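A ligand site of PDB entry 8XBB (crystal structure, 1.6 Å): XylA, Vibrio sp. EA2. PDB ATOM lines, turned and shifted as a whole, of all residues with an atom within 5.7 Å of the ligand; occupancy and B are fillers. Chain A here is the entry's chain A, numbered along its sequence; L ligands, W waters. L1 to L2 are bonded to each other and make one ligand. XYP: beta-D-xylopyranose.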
ATOM      1  N   ILE A  35      -2.694   2.443 -12.545  1.00  0.00           N
ATOM      2  CA  ILE A  35      -3.033   3.845 -12.676  1.00  0.00           C
ATOM      3  C   ILE A  35      -2.153   4.792 -11.846  1.00  0.00           C
ATOM      4  O   ILE A  35      -2.529   5.915 -11.592  1.00  0.00           O
ATOM      5  CB  ILE A  35      -4.504   4.074 -12.315  1.00  0.00           C
ATOM      6  CG1 ILE A  35      -4.783   3.779 -10.853  1.00  0.00           C
ATOM      7  CG2 ILE A  35      -5.395   3.215 -13.204  1.00  0.00           C
ATOM      8  CD1 ILE A  35      -6.123   4.314 -10.412  1.00  0.00           C
ATOM      9  N   ASN A  68      -6.180   6.896 -14.729  1.00  0.00           N
ATOM     10  CA  ASN A  68      -7.465   6.467 -14.145  1.00  0.00           C
ATOM     11  C   ASN A  68      -8.683   6.491 -15.057  1.00  0.00           C
ATOM     12  O   ASN A  68      -9.308   5.503 -15.249  1.00  0.00           O
ATOM     13  CB  ASN A  68      -7.690   7.286 -12.860  1.00  0.00           C
ATOM     14  CG  ASN A  68      -8.925   6.941 -12.094  1.00  0.00           C
ATOM     15  OD1 ASN A  68      -9.215   5.808 -11.815  1.00  0.00           O
ATOM     16  ND2 ASN A  68      -9.651   7.968 -11.696  1.00  0.00           N
ATOM     17  N   GLU A  69      -9.032   7.688 -15.524  1.00  0.00           N
ATOM     18  CA  GLU A  69     -10.252   7.772 -16.328  1.00  0.00           C
ATOM     19  C   GLU A  69     -10.115   6.966 -17.625  1.00  0.00           C
ATOM     20  O   GLU A  69     -11.049   6.250 -18.014  1.00  0.00           O
ATOM     21  CB  GLU A  69     -10.588   9.230 -16.628  1.00  0.00           C
ATOM     22  CG  GLU A  69     -11.082  10.019 -15.422  1.00  0.00           C
ATOM     23  CD  GLU A  69     -12.253   9.354 -14.733  1.00  0.00           C
ATOM     24  OE1 GLU A  69     -12.171   9.148 -13.500  1.00  0.00           O
ATOM     25  OE2 GLU A  69     -13.271   9.052 -15.401  1.00  0.00           O
ATOM     26  N   LYS A  72     -10.405   3.073 -16.822  1.00  0.00           N
ATOM     27  CA  LYS A  72     -11.702   2.561 -16.576  1.00  0.00           C
ATOM     28  C   LYS A  72     -12.474   2.456 -17.902  1.00  0.00           C
ATOM     29  O   LYS A  72     -13.237   1.550 -18.108  1.00  0.00           O
ATOM     30  CB  LYS A  72     -12.482   3.425 -15.577  1.00  0.00           C
ATOM     31  CG  LYS A  72     -11.911   3.384 -14.164  1.00  0.00           C
ATOM     32  CD  LYS A  72     -12.703   4.240 -13.195  1.00  0.00           C
ATOM     33  CE  LYS A  72     -12.525   5.718 -13.439  1.00  0.00           C
ATOM     34  NZ  LYS A  72     -13.225   6.513 -12.396  1.00  0.00           N
ATOM     35  N   TYR A  89      -5.338  -3.158 -12.266  1.00  0.00           N
ATOM     36  CA  TYR A  89      -5.861  -2.510 -11.067  1.00  0.00           C
ATOM     37  C   TYR A  89      -7.367  -2.695 -10.956  1.00  0.00           C
ATOM     38  O   TYR A  89      -8.089  -2.621 -11.956  1.00  0.00           O
ATOM     39  CB  TYR A  89      -5.510  -1.030 -11.099  1.00  0.00           C
ATOM     40  CG  TYR A  89      -5.658  -0.274  -9.798  1.00  0.00           C
ATOM     41  CD1 TYR A  89      -4.751  -0.452  -8.757  1.00  0.00           C
ATOM     42  CD2 TYR A  89      -6.669   0.668  -9.628  1.00  0.00           C
ATOM     43  CE1 TYR A  89      -4.864   0.253  -7.587  1.00  0.00           C
ATOM     44  CE2 TYR A  89      -6.780   1.370  -8.444  1.00  0.00           C
ATOM     45  CZ  TYR A  89      -5.878   1.165  -7.437  1.00  0.00           C
ATOM     46  OH  TYR A  89      -5.968   1.890  -6.264  1.00  0.00           O
ATOM     47  N   TRP A  91     -10.960  -2.148  -8.212  1.00  0.00           N
ATOM     48  CA  TRP A  91     -11.593  -1.666  -7.005  1.00  0.00           C
ATOM     49  C   TRP A  91     -12.467  -2.726  -6.349  1.00  0.00           C
ATOM     50  O   TRP A  91     -13.123  -2.435  -5.336  1.00  0.00           O
ATOM     51  CB  TRP A  91     -12.420  -0.411  -7.303  1.00  0.00           C
ATOM     52  CG  TRP A  91     -11.607   0.801  -7.702  1.00  0.00           C
ATOM     53  CD1 TRP A  91     -11.171   1.798  -6.882  1.00  0.00           C
ATOM     54  CD2 TRP A  91     -11.121   1.129  -9.020  1.00  0.00           C
ATOM     55  NE1 TRP A  91     -10.443   2.728  -7.599  1.00  0.00           N
ATOM     56  CE2 TRP A  91     -10.415   2.338  -8.917  1.00  0.00           C
ATOM     57  CE3 TRP A  91     -11.243   0.522 -10.280  1.00  0.00           C
ATOM     58  CZ2 TRP A  91      -9.814   2.953 -10.021  1.00  0.00           C
ATOM     59  CZ3 TRP A  91     -10.632   1.129 -11.380  1.00  0.00           C
ATOM     60  CH2 TRP A  91      -9.933   2.336 -11.240  1.00  0.00           C
ATOM     61  N   MET A 139      -4.288  -2.227  -1.029  1.00  0.00           N
ATOM     62  CA  MET A 139      -4.452  -1.213  -0.025  1.00  0.00           C
ATOM     63  C   MET A 139      -5.886  -0.982   0.428  1.00  0.00           C
ATOM     64  O   MET A 139      -6.814  -1.396  -0.228  1.00  0.00           O
ATOM     65  CB  MET A 139      -3.958   0.120  -0.560  1.00  0.00           C
ATOM     66  CG  MET A 139      -4.714   0.599  -1.771  1.00  0.00           C
ATOM     67  SD  MET A 139      -4.332   2.296  -2.172  1.00  0.00           S
ATOM     68  CE  MET A 139      -5.971   2.965  -2.454  1.00  0.00           C
ATOM     69  N   SER A 141      -8.401   2.253   2.108  1.00  0.00           N
ATOM     70  CA  SER A 141      -8.373   3.708   2.068  1.00  0.00           C
ATOM     71  C   SER A 141      -9.577   4.259   2.828  1.00  0.00           C
ATOM     72  O   SER A 141     -10.561   3.549   3.070  1.00  0.00           O
ATOM     73  CB  SER A 141      -8.366   4.235   0.622  1.00  0.00           C
ATOM     74  OG  SER A 141      -9.562   3.904  -0.073  1.00  0.00           O
ATOM     75  N   TRP A 191     -16.558  11.654 -10.136  1.00  0.00           N
ATOM     76  CA  TRP A 191     -16.464  10.871  -8.916  1.00  0.00           C
ATOM     77  C   TRP A 191     -16.001  11.675  -7.690  1.00  0.00           C
ATOM     78  O   TRP A 191     -16.448  11.328  -6.583  1.00  0.00           O
ATOM     79  CB  TRP A 191     -15.598   9.598  -9.134  1.00  0.00           C
ATOM     80  CG  TRP A 191     -14.151   9.842  -9.525  1.00  0.00           C
ATOM     81  CD1 TRP A 191     -13.642   9.835 -10.790  1.00  0.00           C
ATOM     82  CD2 TRP A 191     -13.052  10.089  -8.644  1.00  0.00           C
ATOM     83  NE1 TRP A 191     -12.294  10.075 -10.759  1.00  0.00           N
ATOM     84  CE2 TRP A 191     -11.904  10.246  -9.452  1.00  0.00           C
ATOM     85  CE3 TRP A 191     -12.931  10.210  -7.253  1.00  0.00           C
ATOM     86  CZ2 TRP A 191     -10.645  10.514  -8.929  1.00  0.00           C
ATOM     87  CZ3 TRP A 191     -11.662  10.470  -6.725  1.00  0.00           C
ATOM     88  CH2 TRP A 191     -10.542  10.623  -7.561  1.00  0.00           C
ATOM     89  N   HIS A 194     -19.138  12.862  -6.236  1.00  0.00           N
ATOM     90  CA  HIS A 194     -19.961  11.810  -5.706  1.00  0.00           C
ATOM     91  C   HIS A 194     -19.617  11.395  -4.294  1.00  0.00           C
ATOM     92  O   HIS A 194     -20.378  10.787  -3.633  1.00  0.00           O
ATOM     93  CB  HIS A 194     -20.068  10.632  -6.695  1.00  0.00           C
ATOM     94  CG  HIS A 194     -19.361   9.372  -6.301  1.00  0.00           C
ATOM     95  ND1 HIS A 194     -17.996   9.254  -6.309  1.00  0.00           N
ATOM     96  CD2 HIS A 194     -19.835   8.145  -5.977  1.00  0.00           C
ATOM     97  CE1 HIS A 194     -17.652   8.032  -5.964  1.00  0.00           C
ATOM     98  NE2 HIS A 194     -18.757   7.339  -5.759  1.00  0.00           N
ATOM     99  N   PHE A 195     -18.427  11.743  -3.885  1.00  0.00           N
ATOM    100  CA  PHE A 195     -18.048  11.454  -2.527  1.00  0.00           C
ATOM    101  C   PHE A 195     -18.970  12.215  -1.554  1.00  0.00           C
ATOM    102  O   PHE A 195     -19.237  11.737  -0.483  1.00  0.00           O
ATOM    103  CB  PHE A 195     -16.607  11.862  -2.227  1.00  0.00           C
ATOM    104  CG  PHE A 195     -15.543  10.983  -2.823  1.00  0.00           C
ATOM    105  CD1 PHE A 195     -15.805   9.729  -3.279  1.00  0.00           C
ATOM    106  CD2 PHE A 195     -14.246  11.434  -2.873  1.00  0.00           C
ATOM    107  CE1 PHE A 195     -14.802   8.950  -3.797  1.00  0.00           C
ATOM    108  CE2 PHE A 195     -13.234  10.670  -3.389  1.00  0.00           C
ATOM    109  CZ  PHE A 195     -13.513   9.420  -3.842  1.00  0.00           C
ATOM    110  N   TYR A 251      -9.441  15.728 -11.437  1.00  0.00           N
ATOM    111  CA  TYR A 251      -8.833  15.477 -10.133  1.00  0.00           C
ATOM    112  C   TYR A 251      -7.458  16.133 -10.004  1.00  0.00           C
ATOM    113  O   TYR A 251      -7.145  16.741  -8.971  1.00  0.00           O
ATOM    114  CB  TYR A 251      -8.784  13.959  -9.903  1.00  0.00           C
ATOM    115  CG  TYR A 251      -8.033  13.495  -8.672  1.00  0.00           C
ATOM    116  CD1 TYR A 251      -8.170  14.145  -7.454  1.00  0.00           C
ATOM    117  CD2 TYR A 251      -7.203  12.373  -8.716  1.00  0.00           C
ATOM    118  CE1 TYR A 251      -7.482  13.727  -6.325  1.00  0.00           C
ATOM    119  CE2 TYR A 251      -6.531  11.936  -7.582  1.00  0.00           C
ATOM    120  CZ  TYR A 251      -6.674  12.624  -6.391  1.00  0.00           C
ATOM    121  OH  TYR A 251      -6.006  12.238  -5.246  1.00  0.00           O
ATOM    122  N   TRP A 271      -4.794   8.798  -0.176  1.00  0.00           N
ATOM    123  CA  TRP A 271      -3.764   8.952  -1.194  1.00  0.00           C
ATOM    124  C   TRP A 271      -3.525  10.413  -1.584  1.00  0.00           C
ATOM    125  O   TRP A 271      -2.522  10.709  -2.247  1.00  0.00           O
ATOM    126  CB  TRP A 271      -4.154   8.135  -2.435  1.00  0.00           C
ATOM    127  CG  TRP A 271      -5.463   8.583  -3.070  1.00  0.00           C
ATOM    128  CD1 TRP A 271      -5.655   9.654  -3.883  1.00  0.00           C
ATOM    129  CD2 TRP A 271      -6.755   7.963  -2.914  1.00  0.00           C
ATOM    130  NE1 TRP A 271      -6.983   9.740  -4.256  1.00  0.00           N
ATOM    131  CE2 TRP A 271      -7.674   8.717  -3.680  1.00  0.00           C
ATOM    132  CE3 TRP A 271      -7.211   6.842  -2.204  1.00  0.00           C
ATOM    133  CZ2 TRP A 271      -9.027   8.395  -3.750  1.00  0.00           C
ATOM    134  CZ3 TRP A 271      -8.559   6.525  -2.280  1.00  0.00           C
ATOM    135  CH2 TRP A 271      -9.445   7.293  -3.053  1.00  0.00           C
ATOM    136  N   ASN A 314      -8.669  -1.767  -2.594  1.00  0.00           N
ATOM    137  CA  ASN A 314      -8.213  -1.792  -3.960  1.00  0.00           C
ATOM    138  C   ASN A 314      -7.164  -2.891  -4.103  1.00  0.00           C
ATOM    139  O   ASN A 314      -6.509  -3.262  -3.121  1.00  0.00           O
ATOM    140  CB  ASN A 314      -7.626  -0.426  -4.349  1.00  0.00           C
ATOM    141  CG  ASN A 314      -8.677   0.680  -4.408  1.00  0.00           C
ATOM    142  OD1 ASN A 314      -9.827   0.511  -3.988  1.00  0.00           O
ATOM    143  ND2 ASN A 314      -8.273   1.814  -4.950  1.00  0.00           N
ATOM    144  N   PHE A 380     -16.559   2.768  -2.311  1.00  0.00           N
ATOM    145  CA  PHE A 380     -17.018   3.864  -3.155  1.00  0.00           C
ATOM    146  C   PHE A 380     -18.281   3.471  -3.888  1.00  0.00           C
ATOM    147  O   PHE A 380     -18.305   2.447  -4.536  1.00  0.00           O
ATOM    148  CB  PHE A 380     -15.948   4.205  -4.199  1.00  0.00           C
ATOM    149  CG  PHE A 380     -14.551   4.333  -3.652  1.00  0.00           C
ATOM    150  CD1 PHE A 380     -14.221   5.369  -2.801  1.00  0.00           C
ATOM    151  CD2 PHE A 380     -13.569   3.430  -4.015  1.00  0.00           C
ATOM    152  CE1 PHE A 380     -12.947   5.499  -2.317  1.00  0.00           C
ATOM    153  CE2 PHE A 380     -12.290   3.547  -3.520  1.00  0.00           C
ATOM    154  CZ  PHE A 380     -11.977   4.587  -2.666  1.00  0.00           C
ATOM    155  N   ASP A 382     -19.657   4.450  -6.616  1.00  0.00           N
ATOM    156  CA  ASP A 382     -19.624   4.227  -8.064  1.00  0.00           C
ATOM    157  C   ASP A 382     -18.950   2.904  -8.379  1.00  0.00           C
ATOM    158  O   ASP A 382     -19.321   2.249  -9.360  1.00  0.00           O
ATOM    159  CB  ASP A 382     -18.973   5.392  -8.824  1.00  0.00           C
ATOM    160  CG  ASP A 382     -17.471   5.546  -8.564  1.00  0.00           C
ATOM    161  OD1 ASP A 382     -16.959   5.092  -7.522  1.00  0.00           O
ATOM    162  OD2 ASP A 382     -16.786   6.154  -9.422  1.00  0.00           O
ATOM    163  N   GLN A 383     -18.034   2.450  -7.539  1.00  0.00           N
ATOM    164  CA  GLN A 383     -17.426   1.139  -7.744  1.00  0.00           C
ATOM    165  C   GLN A 383     -18.296   0.013  -7.212  1.00  0.00           C
ATOM    166  O   GLN A 383     -18.305  -1.091  -7.778  1.00  0.00           O
ATOM    167  CB  GLN A 383     -16.049   1.101  -7.095  1.00  0.00           C
ATOM    168  CG  GLN A 383     -15.084   2.100  -7.721  1.00  0.00           C
ATOM    169  CD  GLN A 383     -14.828   1.791  -9.185  1.00  0.00           C
ATOM    170  OE1 GLN A 383     -14.955   0.637  -9.608  1.00  0.00           O
ATOM    171  NE2 GLN A 383     -14.455   2.794  -9.951  1.00  0.00           N
ATOM    172  N   ASN A 394     -22.522   9.120 -10.300  1.00  0.00           N
ATOM    173  CA  ASN A 394     -21.588  10.197 -10.630  1.00  0.00           C
ATOM    174  C   ASN A 394     -22.289  11.328 -11.373  1.00  0.00           C
ATOM    175  O   ASN A 394     -22.082  12.511 -11.067  1.00  0.00           O
ATOM    176  CB  ASN A 394     -20.422   9.625 -11.450  1.00  0.00           C
ATOM    177  CG  ASN A 394     -19.394   8.903 -10.598  1.00  0.00           C
ATOM    178  OD1 ASN A 394     -19.365   9.066  -9.379  1.00  0.00           O
ATOM    179  ND2 ASN A 394     -18.547   8.096 -11.241  1.00  0.00           N
HETATM  180  O1  XYP L   1      -5.169   7.729  -7.909  1.00  0.00           O
HETATM  181  C1  XYP L   1      -6.247   7.252  -7.084  1.00  0.00           C
HETATM  182  C2  XYP L   1      -7.441   6.976  -7.992  1.00  0.00           C
HETATM  183  C3  XYP L   1      -8.573   6.348  -7.218  1.00  0.00           C
HETATM  184  C4  XYP L   1      -8.032   5.140  -6.457  1.00  0.00           C
HETATM  185  C5  XYP L   1      -6.863   5.537  -5.585  1.00  0.00           C
HETATM  186  O2  XYP L   1      -7.892   8.223  -8.505  1.00  0.00           O
HETATM  187  O3  XYP L   1      -9.531   5.915  -8.102  1.00  0.00           O
HETATM  188  O4  XYP L   1      -9.052   4.573  -5.621  1.00  0.00           O
HETATM  189  O5  XYP L   1      -5.838   6.054  -6.433  1.00  0.00           O
HETATM  190  C1  XYP L   2     -10.846   6.425  -7.828  1.00  0.00           C
HETATM  191  C2  XYP L   2     -11.830   5.886  -8.857  1.00  0.00           C
HETATM  192  C3  XYP L   2     -13.248   6.330  -8.525  1.00  0.00           C
HETATM  193  C4  XYP L   2     -13.569   5.968  -7.082  1.00  0.00           C
HETATM  194  C5  XYP L   2     -12.492   6.483  -6.117  1.00  0.00           C
HETATM  195  O2  XYP L   2     -11.486   6.363 -10.152  1.00  0.00           O
HETATM  196  O3  XYP L   2     -14.174   5.719  -9.443  1.00  0.00           O
HETATM  197  O4  XYP L   2     -14.812   6.547  -6.705  1.00  0.00           O
HETATM  198  O5  XYP L   2     -11.217   5.999  -6.512  1.00  0.00           O
HETATM  199  O   HOH W   1      -5.759   9.145 -10.589  1.00  0.00           O
HETATM  200  O   HOH W   2      -3.763  10.090  -6.718  1.00  0.00           O
HETATM  201  O   HOH W   3      -3.008   6.450  -5.400  1.00  0.00           O
HETATM  202  O   HOH W   4     -16.093   5.516 -12.086  1.00  0.00           O
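NE2 of Gln 383 sits at hydrogen-bond distance from O3 of XYP L2 (3.0 Å). OD1 of Asn 68 lies within hydrogen-bond range of O2 of XYP L2. An oxygen (O2) of XYP L2 lies within hydrogen-bond range of the side-chain amino group (NZ) of Lys 72. OD2 of Asp 382 sits at hydrogen-bond distance from O3 of XYP L2, 2.6 Å away. The indole nitrogen (NE1) of Trp 91 is in hydrogen-bond range of an oxygen (O4) of XYP L1, 3.0 Å away. The side-chain amide nitrogen of Asn 314 is in hydrogen-bond range of an oxygen (O4) of XYP L1, 2.9 Å away.
Residues that only touch the ligand: His 194, Trp 191, Trp 271, Phe 380, Phe 195, Tyr 89 and Ile 35. Hydrophobic or aromatic side chains within 4 Å of the ligand: Ile 35, Trp 91, Trp 191, His 194, Phe 195, Trp 271 and Phe 380. Of the 18 residues printed, 13 come within 4 Å of the ligand. The nearest printed residue that does not touch the ligand is Tyr 251 (4.1 Å).
O of Trp 191 is in hydrogen-bond range of ND1 of His 194, 2.6 Å away. N of Asn 314 sits at hydrogen-bond distance from O of Met 139. The backbone NH of Asp 382 sits at hydrogen-bond distance from a ring nitrogen (NE2) of His 194 (3.1 Å). The side-chain hydroxyl (OH) of Tyr 89 is in hydrogen-bond range of the side-chain amide nitrogen (ND2) of Asn 314, at 2.7 Å. OD1 of Asn 394 sits close to ND1 of His 194. ND2 of Asn 68 sits at hydrogen-bond distance from OE1 of Glu 69, 3.3 Å away. OD2 of Asp 382 sits at hydrogen-bond distance from ND2 of Asn 394, at 3.2 Å. OE1 of Glu 69 lies within salt-bridge range of NZ of Lys 72 (3.0 Å).
Water W2 lies within hydrogen-bond range of O1 of XYP L1 and OH of Tyr 251. Water W4 lies within hydrogen-bond range of the side-chain carboxylate (OD2) of Asp 382 (2.8 Å), the side-chain amino group (NZ) of Lys 72 (3.1 Å) and an oxygen (O3) of XYP L2 (3.3 Å).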
